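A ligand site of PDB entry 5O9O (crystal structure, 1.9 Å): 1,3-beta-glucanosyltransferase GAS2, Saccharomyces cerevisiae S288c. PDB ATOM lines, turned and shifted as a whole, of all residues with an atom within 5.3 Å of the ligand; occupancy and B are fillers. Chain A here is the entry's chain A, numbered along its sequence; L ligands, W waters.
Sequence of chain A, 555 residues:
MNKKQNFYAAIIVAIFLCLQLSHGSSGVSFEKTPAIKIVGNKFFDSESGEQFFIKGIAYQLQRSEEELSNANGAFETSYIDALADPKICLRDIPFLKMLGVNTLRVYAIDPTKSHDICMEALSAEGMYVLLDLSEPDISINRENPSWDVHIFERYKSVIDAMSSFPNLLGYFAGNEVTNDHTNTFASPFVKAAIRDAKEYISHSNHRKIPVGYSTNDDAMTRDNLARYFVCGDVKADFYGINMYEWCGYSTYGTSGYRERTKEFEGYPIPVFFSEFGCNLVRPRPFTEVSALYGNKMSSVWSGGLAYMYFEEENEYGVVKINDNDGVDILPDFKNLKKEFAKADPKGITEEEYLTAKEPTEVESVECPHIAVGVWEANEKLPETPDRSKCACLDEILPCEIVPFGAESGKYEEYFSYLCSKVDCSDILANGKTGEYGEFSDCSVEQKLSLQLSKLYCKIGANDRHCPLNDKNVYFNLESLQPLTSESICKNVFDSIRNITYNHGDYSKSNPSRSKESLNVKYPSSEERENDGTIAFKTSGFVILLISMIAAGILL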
ATOM      1  N   GLN A  60     -31.714 -19.134  21.676  1.00  0.00           N
ATOM      2  CA  GLN A  60     -30.418 -18.611  22.106  1.00  0.00           C
ATOM      3  C   GLN A  60     -29.574 -18.162  20.913  1.00  0.00           C
ATOM      4  O   GLN A  60     -29.358 -18.914  19.956  1.00  0.00           O
ATOM      5  CB  GLN A  60     -29.652 -19.669  22.922  1.00  0.00           C
ATOM      6  CG  GLN A  60     -28.380 -19.178  23.566  1.00  0.00           C
ATOM      7  CD  GLN A  60     -28.627 -18.437  24.855  1.00  0.00           C
ATOM      8  OE1 GLN A  60     -29.395 -18.888  25.703  1.00  0.00           O
ATOM      9  NE2 GLN A  60     -27.979 -17.287  25.028  1.00  0.00           N
ATOM     10  N   GLN A  62     -26.007 -16.765  19.216  1.00  0.00           N
ATOM     11  CA  GLN A  62     -24.565 -16.828  19.449  1.00  0.00           C
ATOM     12  C   GLN A  62     -23.881 -15.669  18.792  1.00  0.00           C
ATOM     13  O   GLN A  62     -23.366 -14.817  19.437  1.00  0.00           O
ATOM     14  CB  GLN A  62     -23.945 -18.113  18.923  1.00  0.00           C
ATOM     15  CG  GLN A  62     -24.540 -19.372  19.447  1.00  0.00           C
ATOM     16  CD  GLN A  62     -24.057 -19.682  20.822  1.00  0.00           C
ATOM     17  OE1 GLN A  62     -22.888 -19.929  21.030  1.00  0.00           O
ATOM     18  NE2 GLN A  62     -24.944 -19.721  21.758  1.00  0.00           N
ATOM     19  N   TYR A 107     -30.021 -21.014  27.355  1.00  0.00           N
ATOM     20  CA  TYR A 107     -28.801 -21.622  27.870  1.00  0.00           C
ATOM     21  C   TYR A 107     -27.949 -20.640  28.663  1.00  0.00           C
ATOM     22  O   TYR A 107     -27.063 -21.052  29.422  1.00  0.00           O
ATOM     23  CB  TYR A 107     -27.974 -22.176  26.712  1.00  0.00           C
ATOM     24  CG  TYR A 107     -28.620 -23.316  25.966  1.00  0.00           C
ATOM     25  CD1 TYR A 107     -29.540 -23.082  24.951  1.00  0.00           C
ATOM     26  CD2 TYR A 107     -28.297 -24.636  26.267  1.00  0.00           C
ATOM     27  CE1 TYR A 107     -30.118 -24.126  24.258  1.00  0.00           C
ATOM     28  CE2 TYR A 107     -28.873 -25.689  25.577  1.00  0.00           C
ATOM     29  CZ  TYR A 107     -29.781 -25.424  24.585  1.00  0.00           C
ATOM     30  OH  TYR A 107     -30.357 -26.477  23.895  1.00  0.00           O
ATOM     31  N   ALA A 108     -28.172 -19.349  28.471  1.00  0.00           N
ATOM     32  CA  ALA A 108     -27.396 -18.353  29.192  1.00  0.00           C
ATOM     33  C   ALA A 108     -28.102 -17.002  29.237  1.00  0.00           C
ATOM     34  O   ALA A 108     -28.555 -16.501  28.209  1.00  0.00           O
ATOM     35  CB  ALA A 108     -26.015 -18.197  28.554  1.00  0.00           C
ATOM     36  N   ASP A 132     -30.688 -22.768  31.935  1.00  0.00           N
ATOM     37  CA  ASP A 132     -29.405 -23.224  32.477  1.00  0.00           C
ATOM     38  C   ASP A 132     -28.812 -22.206  33.447  1.00  0.00           C
ATOM     39  O   ASP A 132     -28.837 -20.997  33.199  1.00  0.00           O
ATOM     40  CB  ASP A 132     -28.412 -23.503  31.342  1.00  0.00           C
ATOM     41  CG  ASP A 132     -28.884 -24.627  30.419  1.00  0.00           C
ATOM     42  OD1 ASP A 132     -29.845 -24.404  29.632  1.00  0.00           O
ATOM     43  OD2 ASP A 132     -28.306 -25.730  30.496  1.00  0.00           O
ATOM     44  N   SER A 134     -25.586 -22.397  34.351  1.00  0.00           N
ATOM     45  CA  SER A 134     -24.196 -22.201  33.921  1.00  0.00           C
ATOM     46  C   SER A 134     -24.102 -21.411  32.620  1.00  0.00           C
ATOM     47  O   SER A 134     -25.091 -21.009  32.033  1.00  0.00           O
ATOM     48  CB  SER A 134     -23.528 -23.561  33.730  1.00  0.00           C
ATOM     49  OG  SER A 134     -24.188 -24.283  32.697  1.00  0.00           O
ATOM     50  N   GLU A 135     -22.868 -21.254  32.157  1.00  0.00           N
ATOM     51  CA  GLU A 135     -22.559 -20.459  30.976  1.00  0.00           C
ATOM     52  C   GLU A 135     -21.212 -21.004  30.467  1.00  0.00           C
ATOM     53  O   GLU A 135     -20.441 -21.527  31.277  1.00  0.00           O
ATOM     54  CB  GLU A 135     -22.538 -18.975  31.353  1.00  0.00           C
ATOM     55  CG  GLU A 135     -21.922 -18.059  30.392  1.00  0.00           C
ATOM     56  CD  GLU A 135     -20.541 -17.620  30.789  1.00  0.00           C
ATOM     57  OE1 GLU A 135     -20.371 -17.003  31.863  1.00  0.00           O
ATOM     58  OE2 GLU A 135     -19.626 -17.889  29.988  1.00  0.00           O
ATOM     59  N   PRO A 136     -20.930 -20.932  29.143  1.00  0.00           N
ATOM     60  CA  PRO A 136     -19.731 -21.623  28.631  1.00  0.00           C
ATOM     61  C   PRO A 136     -18.437 -21.341  29.383  1.00  0.00           C
ATOM     62  O   PRO A 136     -17.612 -22.243  29.530  1.00  0.00           O
ATOM     63  CB  PRO A 136     -19.645 -21.111  27.185  1.00  0.00           C
ATOM     64  CG  PRO A 136     -21.105 -20.933  26.806  1.00  0.00           C
ATOM     65  CD  PRO A 136     -21.742 -20.361  28.047  1.00  0.00           C
ATOM     66  N   ASP A 137     -18.264 -20.123  29.895  1.00  0.00           N
ATOM     67  CA  ASP A 137     -17.057 -19.784  30.626  1.00  0.00           C
ATOM     68  C   ASP A 137     -17.160 -19.995  32.125  1.00  0.00           C
ATOM     69  O   ASP A 137     -16.165 -19.833  32.845  1.00  0.00           O
ATOM     70  CB  ASP A 137     -16.657 -18.344  30.350  1.00  0.00           C
ATOM     71  CG  ASP A 137     -16.368 -18.093  28.896  1.00  0.00           C
ATOM     72  OD1 ASP A 137     -15.805 -18.999  28.245  1.00  0.00           O
ATOM     73  OD2 ASP A 137     -16.710 -17.008  28.386  1.00  0.00           O
ATOM     74  N   SER A 139     -18.866 -23.060  34.138  1.00  0.00           N
ATOM     75  CA  SER A 139     -19.554 -24.339  34.111  1.00  0.00           C
ATOM     76  C   SER A 139     -18.692 -25.326  34.864  1.00  0.00           C
ATOM     77  O   SER A 139     -17.514 -25.092  35.028  1.00  0.00           O
ATOM     78  CB  SER A 139     -19.770 -24.846  32.672  1.00  0.00           C
ATOM     79  OG  SER A 139     -20.722 -24.069  31.978  1.00  0.00           O
ATOM     80  N   ILE A 140     -19.274 -26.434  35.307  1.00  0.00           N
ATOM     81  CA  ILE A 140     -18.450 -27.504  35.840  1.00  0.00           C
ATOM     82  C   ILE A 140     -17.633 -28.097  34.702  1.00  0.00           C
ATOM     83  O   ILE A 140     -18.195 -28.604  33.734  1.00  0.00           O
ATOM     84  CB  ILE A 140     -19.345 -28.570  36.529  1.00  0.00           C
ATOM     85  CG1 ILE A 140     -20.072 -27.929  37.713  1.00  0.00           C
ATOM     86  CG2 ILE A 140     -18.506 -29.776  36.985  1.00  0.00           C
ATOM     87  CD1 ILE A 140     -21.080 -28.839  38.373  1.00  0.00           C
ATOM     88  N   ASN A 141     -16.313 -27.971  34.772  1.00  0.00           N
ATOM     89  CA  ASN A 141     -15.423 -28.448  33.712  1.00  0.00           C
ATOM     90  C   ASN A 141     -15.324 -29.970  33.696  1.00  0.00           C
ATOM     91  O   ASN A 141     -14.731 -30.567  34.595  1.00  0.00           O
ATOM     92  CB  ASN A 141     -14.040 -27.816  33.882  1.00  0.00           C
ATOM     93  CG  ASN A 141     -13.038 -28.209  32.788  1.00  0.00           C
ATOM     94  OD1 ASN A 141     -13.296 -29.089  31.963  1.00  0.00           O
ATOM     95  ND2 ASN A 141     -11.887 -27.553  32.798  1.00  0.00           N
ATOM     96  N   ARG A 142     -15.884 -30.600  32.667  1.00  0.00           N
ATOM     97  CA  ARG A 142     -15.979 -32.052  32.659  1.00  0.00           C
ATOM     98  C   ARG A 142     -14.606 -32.712  32.588  1.00  0.00           C
ATOM     99  O   ARG A 142     -14.454 -33.857  32.984  1.00  0.00           O
ATOM    100  CB  ARG A 142     -16.872 -32.547  31.506  1.00  0.00           C
ATOM    101  CG  ARG A 142     -16.297 -32.366  30.072  1.00  0.00           C
ATOM    102  CD  ARG A 142     -17.159 -33.063  29.007  1.00  0.00           C
ATOM    103  NE  ARG A 142     -18.497 -32.490  28.854  1.00  0.00           N
ATOM    104  CZ  ARG A 142     -18.786 -31.476  28.046  1.00  0.00           C
ATOM    105  NH1 ARG A 142     -17.823 -30.908  27.318  1.00  0.00           N
ATOM    106  NH2 ARG A 142     -20.031 -31.025  27.944  1.00  0.00           N
ATOM    107  N   GLU A 143     -13.591 -31.994  32.114  1.00  0.00           N
ATOM    108  CA  GLU A 143     -12.236 -32.545  32.065  1.00  0.00           C
ATOM    109  C   GLU A 143     -11.461 -32.351  33.360  1.00  0.00           C
ATOM    110  O   GLU A 143     -10.446 -32.998  33.589  1.00  0.00           O
ATOM    111  CB  GLU A 143     -11.433 -31.901  30.921  1.00  0.00           C
ATOM    112  CG  GLU A 143     -12.200 -31.732  29.613  1.00  0.00           C
ATOM    113  CD  GLU A 143     -12.486 -33.060  28.935  1.00  0.00           C
ATOM    114  OE1 GLU A 143     -11.920 -34.090  29.355  1.00  0.00           O
ATOM    115  OE2 GLU A 143     -13.289 -33.083  27.966  1.00  0.00           O
ATOM    116  N   ASN A 175     -25.339 -29.251  31.988  1.00  0.00           N
ATOM    117  CA  ASN A 175     -25.750 -29.731  30.672  1.00  0.00           C
ATOM    118  C   ASN A 175     -24.683 -30.667  30.100  1.00  0.00           C
ATOM    119  O   ASN A 175     -23.555 -30.225  29.833  1.00  0.00           O
ATOM    120  CB  ASN A 175     -25.998 -28.555  29.720  1.00  0.00           C
ATOM    121  CG  ASN A 175     -26.486 -29.010  28.340  1.00  0.00           C
ATOM    122  OD1 ASN A 175     -27.526 -29.656  28.221  1.00  0.00           O
ATOM    123  ND2 ASN A 175     -25.744 -28.652  27.297  1.00  0.00           N
ATOM    124  N   GLU A 176     -25.016 -31.951  29.956  1.00  0.00           N
ATOM    125  CA  GLU A 176     -24.065 -32.959  29.425  1.00  0.00           C
ATOM    126  C   GLU A 176     -22.669 -32.862  30.037  1.00  0.00           C
ATOM    127  O   GLU A 176     -21.674 -32.769  29.302  1.00  0.00           O
ATOM    128  CB  GLU A 176     -23.940 -32.832  27.908  1.00  0.00           C
ATOM    129  CG  GLU A 176     -25.250 -32.661  27.180  1.00  0.00           C
ATOM    130  CD  GLU A 176     -25.098 -32.635  25.660  1.00  0.00           C
ATOM    131  OE1 GLU A 176     -24.070 -32.125  25.160  1.00  0.00           O
ATOM    132  OE2 GLU A 176     -26.011 -33.112  24.968  1.00  0.00           O
ATOM    133  N   VAL A 177     -22.571 -32.850  31.349  1.00  0.00           N
ATOM    134  CA  VAL A 177     -21.269 -32.671  31.994  1.00  0.00           C
ATOM    135  C   VAL A 177     -20.453 -33.962  31.797  1.00  0.00           C
ATOM    136  O   VAL A 177     -19.546 -34.002  30.976  1.00  0.00           O
ATOM    137  CB  VAL A 177     -21.471 -32.265  33.458  1.00  0.00           C
ATOM    138  CG1 VAL A 177     -20.159 -31.970  34.126  1.00  0.00           C
ATOM    139  CG2 VAL A 177     -22.411 -31.008  33.499  1.00  0.00           C
ATOM    140  N   TYR A 244     -31.667 -37.231  19.784  1.00  0.00           N
ATOM    141  CA  TYR A 244     -31.584 -37.066  18.326  1.00  0.00           C
ATOM    142  C   TYR A 244     -31.747 -38.389  17.552  1.00  0.00           C
ATOM    143  O   TYR A 244     -31.383 -38.475  16.390  1.00  0.00           O
ATOM    144  CB  TYR A 244     -30.259 -36.390  17.950  1.00  0.00           C
ATOM    145  CG  TYR A 244     -30.219 -34.941  18.411  1.00  0.00           C
ATOM    146  CD1 TYR A 244     -29.828 -34.622  19.706  1.00  0.00           C
ATOM    147  CD2 TYR A 244     -30.615 -33.912  17.570  1.00  0.00           C
ATOM    148  CE1 TYR A 244     -29.831 -33.285  20.152  1.00  0.00           C
ATOM    149  CE2 TYR A 244     -30.623 -32.594  17.989  1.00  0.00           C
ATOM    150  CZ  TYR A 244     -30.220 -32.285  19.277  1.00  0.00           C
ATOM    151  OH  TYR A 244     -30.203 -30.984  19.692  1.00  0.00           O
ATOM    152  N   GLU A 275     -33.680 -31.362  24.219  1.00  0.00           N
ATOM    153  CA  GLU A 275     -33.471 -31.045  22.803  1.00  0.00           C
ATOM    154  C   GLU A 275     -33.999 -32.197  21.946  1.00  0.00           C
ATOM    155  O   GLU A 275     -33.843 -33.356  22.326  1.00  0.00           O
ATOM    156  CB  GLU A 275     -31.987 -30.820  22.466  1.00  0.00           C
ATOM    157  CG  GLU A 275     -31.284 -29.660  23.190  1.00  0.00           C
ATOM    158  CD  GLU A 275     -29.761 -29.662  22.925  1.00  0.00           C
ATOM    159  OE1 GLU A 275     -29.281 -30.481  22.090  1.00  0.00           O
ATOM    160  OE2 GLU A 275     -29.054 -28.832  23.539  1.00  0.00           O
ATOM    161  N   TYR A 307     -34.699 -28.237  18.835  1.00  0.00           N
ATOM    162  CA  TYR A 307     -33.466 -27.455  18.725  1.00  0.00           C
ATOM    163  C   TYR A 307     -33.291 -27.046  17.251  1.00  0.00           C
ATOM    164  O   TYR A 307     -33.162 -27.945  16.420  1.00  0.00           O
ATOM    165  CB  TYR A 307     -32.254 -28.267  19.210  1.00  0.00           C
ATOM    166  CG  TYR A 307     -30.994 -27.436  19.213  1.00  0.00           C
ATOM    167  CD1 TYR A 307     -30.185 -27.367  18.076  1.00  0.00           C
ATOM    168  CD2 TYR A 307     -30.650 -26.657  20.321  1.00  0.00           C
ATOM    169  CE1 TYR A 307     -29.049 -26.573  18.059  1.00  0.00           C
ATOM    170  CE2 TYR A 307     -29.524 -25.863  20.314  1.00  0.00           C
ATOM    171  CZ  TYR A 307     -28.728 -25.827  19.184  1.00  0.00           C
ATOM    172  OH  TYR A 307     -27.604 -25.024  19.174  1.00  0.00           O
ATOM    173  N   MET A 308     -33.307 -25.750  16.887  1.00  0.00           N
ATOM    174  CA  MET A 308     -33.666 -24.609  17.762  1.00  0.00           C
ATOM    175  C   MET A 308     -34.300 -23.502  16.922  1.00  0.00           C
ATOM    176  O   MET A 308     -34.476 -23.657  15.705  1.00  0.00           O
ATOM    177  CB  MET A 308     -32.445 -24.044  18.486  1.00  0.00           C
ATOM    178  CG  MET A 308     -31.483 -23.267  17.588  1.00  0.00           C
ATOM    179  SD  MET A 308     -30.547 -21.979  18.473  1.00  0.00           S
ATOM    180  CE  MET A 308     -31.813 -20.793  18.943  1.00  0.00           C
ATOM    181  N   GLU A 312     -28.079 -20.936  12.572  1.00  0.00           N
ATOM    182  CA  GLU A 312     -26.707 -20.457  12.740  1.00  0.00           C
ATOM    183  C   GLU A 312     -25.684 -21.338  12.025  1.00  0.00           C
ATOM    184  O   GLU A 312     -24.729 -21.808  12.628  1.00  0.00           O
ATOM    185  CB  GLU A 312     -26.380 -20.376  14.237  1.00  0.00           C
ATOM    186  CG  GLU A 312     -27.236 -19.344  14.956  1.00  0.00           C
ATOM    187  CD  GLU A 312     -26.995 -19.290  16.434  1.00  0.00           C
ATOM    188  OE1 GLU A 312     -26.841 -18.159  16.956  1.00  0.00           O
ATOM    189  OE2 GLU A 312     -26.968 -20.361  17.092  1.00  0.00           O
ATOM    190  N   TYR A 316     -29.850 -25.995  12.109  1.00  0.00           N
ATOM    191  CA  TYR A 316     -30.843 -26.422  13.098  1.00  0.00           C
ATOM    192  C   TYR A 316     -31.963 -25.392  13.299  1.00  0.00           C
ATOM    193  O   TYR A 316     -32.869 -25.630  14.079  1.00  0.00           O
ATOM    194  CB  TYR A 316     -30.200 -26.751  14.448  1.00  0.00           C
ATOM    195  CG  TYR A 316     -29.450 -28.076  14.452  1.00  0.00           C
ATOM    196  CD1 TYR A 316     -30.117 -29.282  14.552  1.00  0.00           C
ATOM    197  CD2 TYR A 316     -28.068 -28.099  14.317  1.00  0.00           C
ATOM    198  CE1 TYR A 316     -29.427 -30.495  14.552  1.00  0.00           C
ATOM    199  CE2 TYR A 316     -27.357 -29.310  14.308  1.00  0.00           C
ATOM    200  CZ  TYR A 316     -28.060 -30.499  14.422  1.00  0.00           C
ATOM    201  OH  TYR A 316     -27.383 -31.699  14.407  1.00  0.00           O
HETATM  202  C1  LIG L   1     -22.798 -24.413  29.044  1.00  0.00           C
HETATM  203  C2  LIG L   1     -24.196 -24.700  28.554  1.00  0.00           C
HETATM  204  C3  LIG L   1     -25.194 -23.800  29.317  1.00  0.00           C
HETATM  205  C4  LIG L   1     -21.840 -25.278  28.289  1.00  0.00           C
HETATM  206  C5  LIG L   1     -26.525 -33.840  18.233  1.00  0.00           C
HETATM  207  C6  LIG L   1     -25.702 -34.965  18.159  1.00  0.00           C
HETATM  208  C7  LIG L   1     -26.135 -36.172  18.681  1.00  0.00           C
HETATM  209  C8  LIG L   1     -25.312 -37.298  18.607  1.00  0.00           C
HETATM  210  C9  LIG L   1     -24.068 -37.212  17.997  1.00  0.00           C
HETATM  211  C10 LIG L   1     -23.634 -36.008  17.464  1.00  0.00           C
HETATM  212  C11 LIG L   1     -24.455 -34.892  17.542  1.00  0.00           C
HETATM  213  C12 LIG L   1     -24.012 -33.685  17.009  1.00  0.00           C
HETATM  214  C13 LIG L   1     -24.832 -32.569  17.086  1.00  0.00           C
HETATM  215  C14 LIG L   1     -26.081 -32.636  17.691  1.00  0.00           C
HETATM  216  C15 LIG L   1     -26.852 -31.472  17.739  1.00  0.00           C
HETATM  217  O1  LIG L   1     -26.399 -30.675  18.850  1.00  0.00           O
HETATM  218  C16 LIG L   1     -26.946 -29.376  18.755  1.00  0.00           C
HETATM  219  C17 LIG L   1     -26.349 -28.456  19.824  1.00  0.00           C
HETATM  220  C18 LIG L   1     -26.978 -27.902  20.843  1.00  0.00           C
HETATM  221  N1  LIG L   1     -25.099 -28.018  19.848  1.00  0.00           N
HETATM  222  N2  LIG L   1     -24.966 -27.297  20.830  1.00  0.00           N
HETATM  223  N3  LIG L   1     -26.008 -27.248  21.503  1.00  0.00           N
HETATM  224  C19 LIG L   1     -26.038 -26.306  22.621  1.00  0.00           C
HETATM  225  C20 LIG L   1     -24.704 -26.172  23.271  1.00  0.00           C
HETATM  226  O2  LIG L   1     -24.512 -27.438  23.920  1.00  0.00           O
HETATM  227  O3  LIG L   1     -26.392 -25.056  22.067  1.00  0.00           O
HETATM  228  C21 LIG L   1     -26.472 -23.995  23.046  1.00  0.00           C
HETATM  229  C22 LIG L   1     -26.512 -22.745  22.164  1.00  0.00           C
HETATM  230  O4  LIG L   1     -27.588 -22.830  21.262  1.00  0.00           O
HETATM  231  C23 LIG L   1     -25.159 -23.860  23.715  1.00  0.00           C
HETATM  232  O5  LIG L   1     -25.302 -22.833  24.708  1.00  0.00           O
HETATM  233  C24 LIG L   1     -24.816 -25.189  24.382  1.00  0.00           C
HETATM  234  O6  LIG L   1     -23.538 -25.039  25.023  1.00  0.00           O
HETATM  235  C25 LIG L   1     -23.422 -25.292  26.406  1.00  0.00           C
HETATM  236  C26 LIG L   1     -21.967 -25.019  26.790  1.00  0.00           C
HETATM  237  O7  LIG L   1     -21.130 -25.939  26.030  1.00  0.00           O
HETATM  238  O8  LIG L   1     -24.315 -24.435  27.147  1.00  0.00           O
HETATM  239  O9  LIG L   1     -24.864 -22.446  29.069  1.00  0.00           O
HETATM  240  O10 LIG L   1     -22.757 -24.851  30.407  1.00  0.00           O
HETATM  241  O11 LIG L   1     -20.512 -25.036  28.723  1.00  0.00           O
HETATM  242  C27 LIG L   1     -19.603 -26.098  28.752  1.00  0.00           C
HETATM  243  O12 LIG L   1     -20.151 -26.961  29.725  1.00  0.00           O
HETATM  244  C28 LIG L   1     -19.318 -28.130  29.902  1.00  0.00           C
HETATM  245  C29 LIG L   1     -20.071 -29.079  30.871  1.00  0.00           C
HETATM  246  O13 LIG L   1     -20.358 -28.422  32.127  1.00  0.00           O
HETATM  247  C30 LIG L   1     -17.921 -27.678  30.369  1.00  0.00           C
HETATM  248  O14 LIG L   1     -17.082 -28.833  30.438  1.00  0.00           O
HETATM  249  C31 LIG L   1     -17.298 -26.747  29.342  1.00  0.00           C
HETATM  250  O15 LIG L   1     -16.114 -26.198  29.891  1.00  0.00           O
HETATM  251  C32 LIG L   1     -18.236 -25.571  29.208  1.00  0.00           C
HETATM  252  O16 LIG L   1     -17.793 -24.588  28.267  1.00  0.00           O
HETATM  253  O   HOH W   1     -24.773 -19.997  24.552  1.00  0.00           O
HETATM  254  O   HOH W   2     -27.496 -20.609  19.833  1.00  0.00           O
HETATM  255  O   HOH W   3     -23.045 -27.482  32.271  1.00  0.00           O
HETATM  256  O   HOH W   4     -22.947 -28.490  27.763  1.00  0.00           O
HETATM  257  O   HOH W   5     -26.991 -31.460  21.303  1.00  0.00           O
HETATM  258  O   HOH W   6     -26.772 -29.410  24.586  1.00  0.00           O
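The backbone carbonyl oxygen (O) of Tyr 107 lies within hydrogen-bond range of an oxygen (O9) of the ligand (2.6 Å). The backbone carbonyl oxygen (O) of Pro 136 lies within hydrogen-bond range of an oxygen (O16) of the ligand (2.7 Å). The side-chain hydroxyl (OG) of Ser 139 sits at hydrogen-bond distance from an oxygen (O10) of the ligand (2.7 Å). An oxygen (O13) of the ligand is in hydrogen-bond range of the backbone carbonyl oxygen of Ile 140, 2.7 Å away. O9 of the ligand is in hydrogen-bond range of O of Ser 134. The side-chain hydroxyl (OG) of Ser 134 sits at hydrogen-bond distance from an oxygen (O10) of the ligand (2.8 Å). OH of Tyr 307 sits at hydrogen-bond distance from O4 of the ligand, at 3.0 Å. An oxygen (O14) of the ligand lies within hydrogen-bond range of the backbone NH (N) of Arg 142.
Water W5 bridges OE1 of Glu 275 (2.6 Å) and O1 of the ligand (2.6 Å). Water W3 lies within hydrogen-bond range of O13 of the ligand (2.9 Å), N of Asn 175 (2.9 Å) and OG of Ser 134 (3.4 Å). Water W1 bridges the side-chain amide nitrogen (NE2) of Gln 62 (2.8 Å) and an oxygen (O5) of the ligand (2.9 Å). Water W6 lies within hydrogen-bond range of OE2 of Glu 275 (2.6 Å), ND2 of Asn 175 (3.0 Å) and O2 of the ligand (3.1 Å).
NE2 of Gln 62 touches C22 of the ligand, 3.4 Å away. Asp 132 touches the ligand (CB to C3, 3.8 Å). CA of Glu 135 touches O9 of the ligand, 3.6 Å away. CA of Asn 141 touches O14 of the ligand (3.7 Å). Asn 175 touches the ligand (ND2 to O2, 3.8 Å). CG2 of Val 177 touches O13 of the ligand, at 3.6 Å. Tyr 244 touches the ligand. Glu 275 touches the ligand. OH of Tyr 316 touches C15 of the ligand (3.4 Å). Hydrophobic or aromatic side chains that line the ligand: Tyr 107, Pro 136, Val 177, Tyr 244, Tyr 307 and Tyr 316. Within 4 Å of the ligand: Gln 62, Tyr 107, Asp 132, Ser 134, Glu 135, Pro 136, Ser 139, Ile 140, Asn 141, Arg 142, Asn 175, Val 177, Tyr 244, Glu 275, Tyr 307 and Tyr 316.
The side-chain hydroxyl (OH) of Tyr 107 sits at hydrogen-bond distance from the side-chain carboxylate (OE2) of Glu 275 (2.7 Å). N of Tyr 107 is in hydrogen-bond range of OE1 of Gln 60 (2.8 Å). The side-chain hydroxyl (OG) of Ser 139 is in hydrogen-bond range of the backbone carbonyl oxygen (O) of Glu 135, 2.7 Å away. The guanidinium group (NE) of Arg 142 is in hydrogen-bond range of the backbone carbonyl oxygen (O) of Val 177, 2.8 Å away. NH2 of Arg 142 sits at hydrogen-bond distance from O of Glu 176, at 2.8 Å. The backbone carbonyl oxygen (O) of Tyr 316 sits at hydrogen-bond distance from the backbone NH (N) of Met 308 (2.8 Å). The backbone NH (N) of Gln 62 is in hydrogen-bond range of the side-chain carboxylate (OE1) of Glu 312. The backbone NH of Glu 143 lies within hydrogen-bond range of the side-chain amide oxygen of Asn 141 (2.9 Å).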
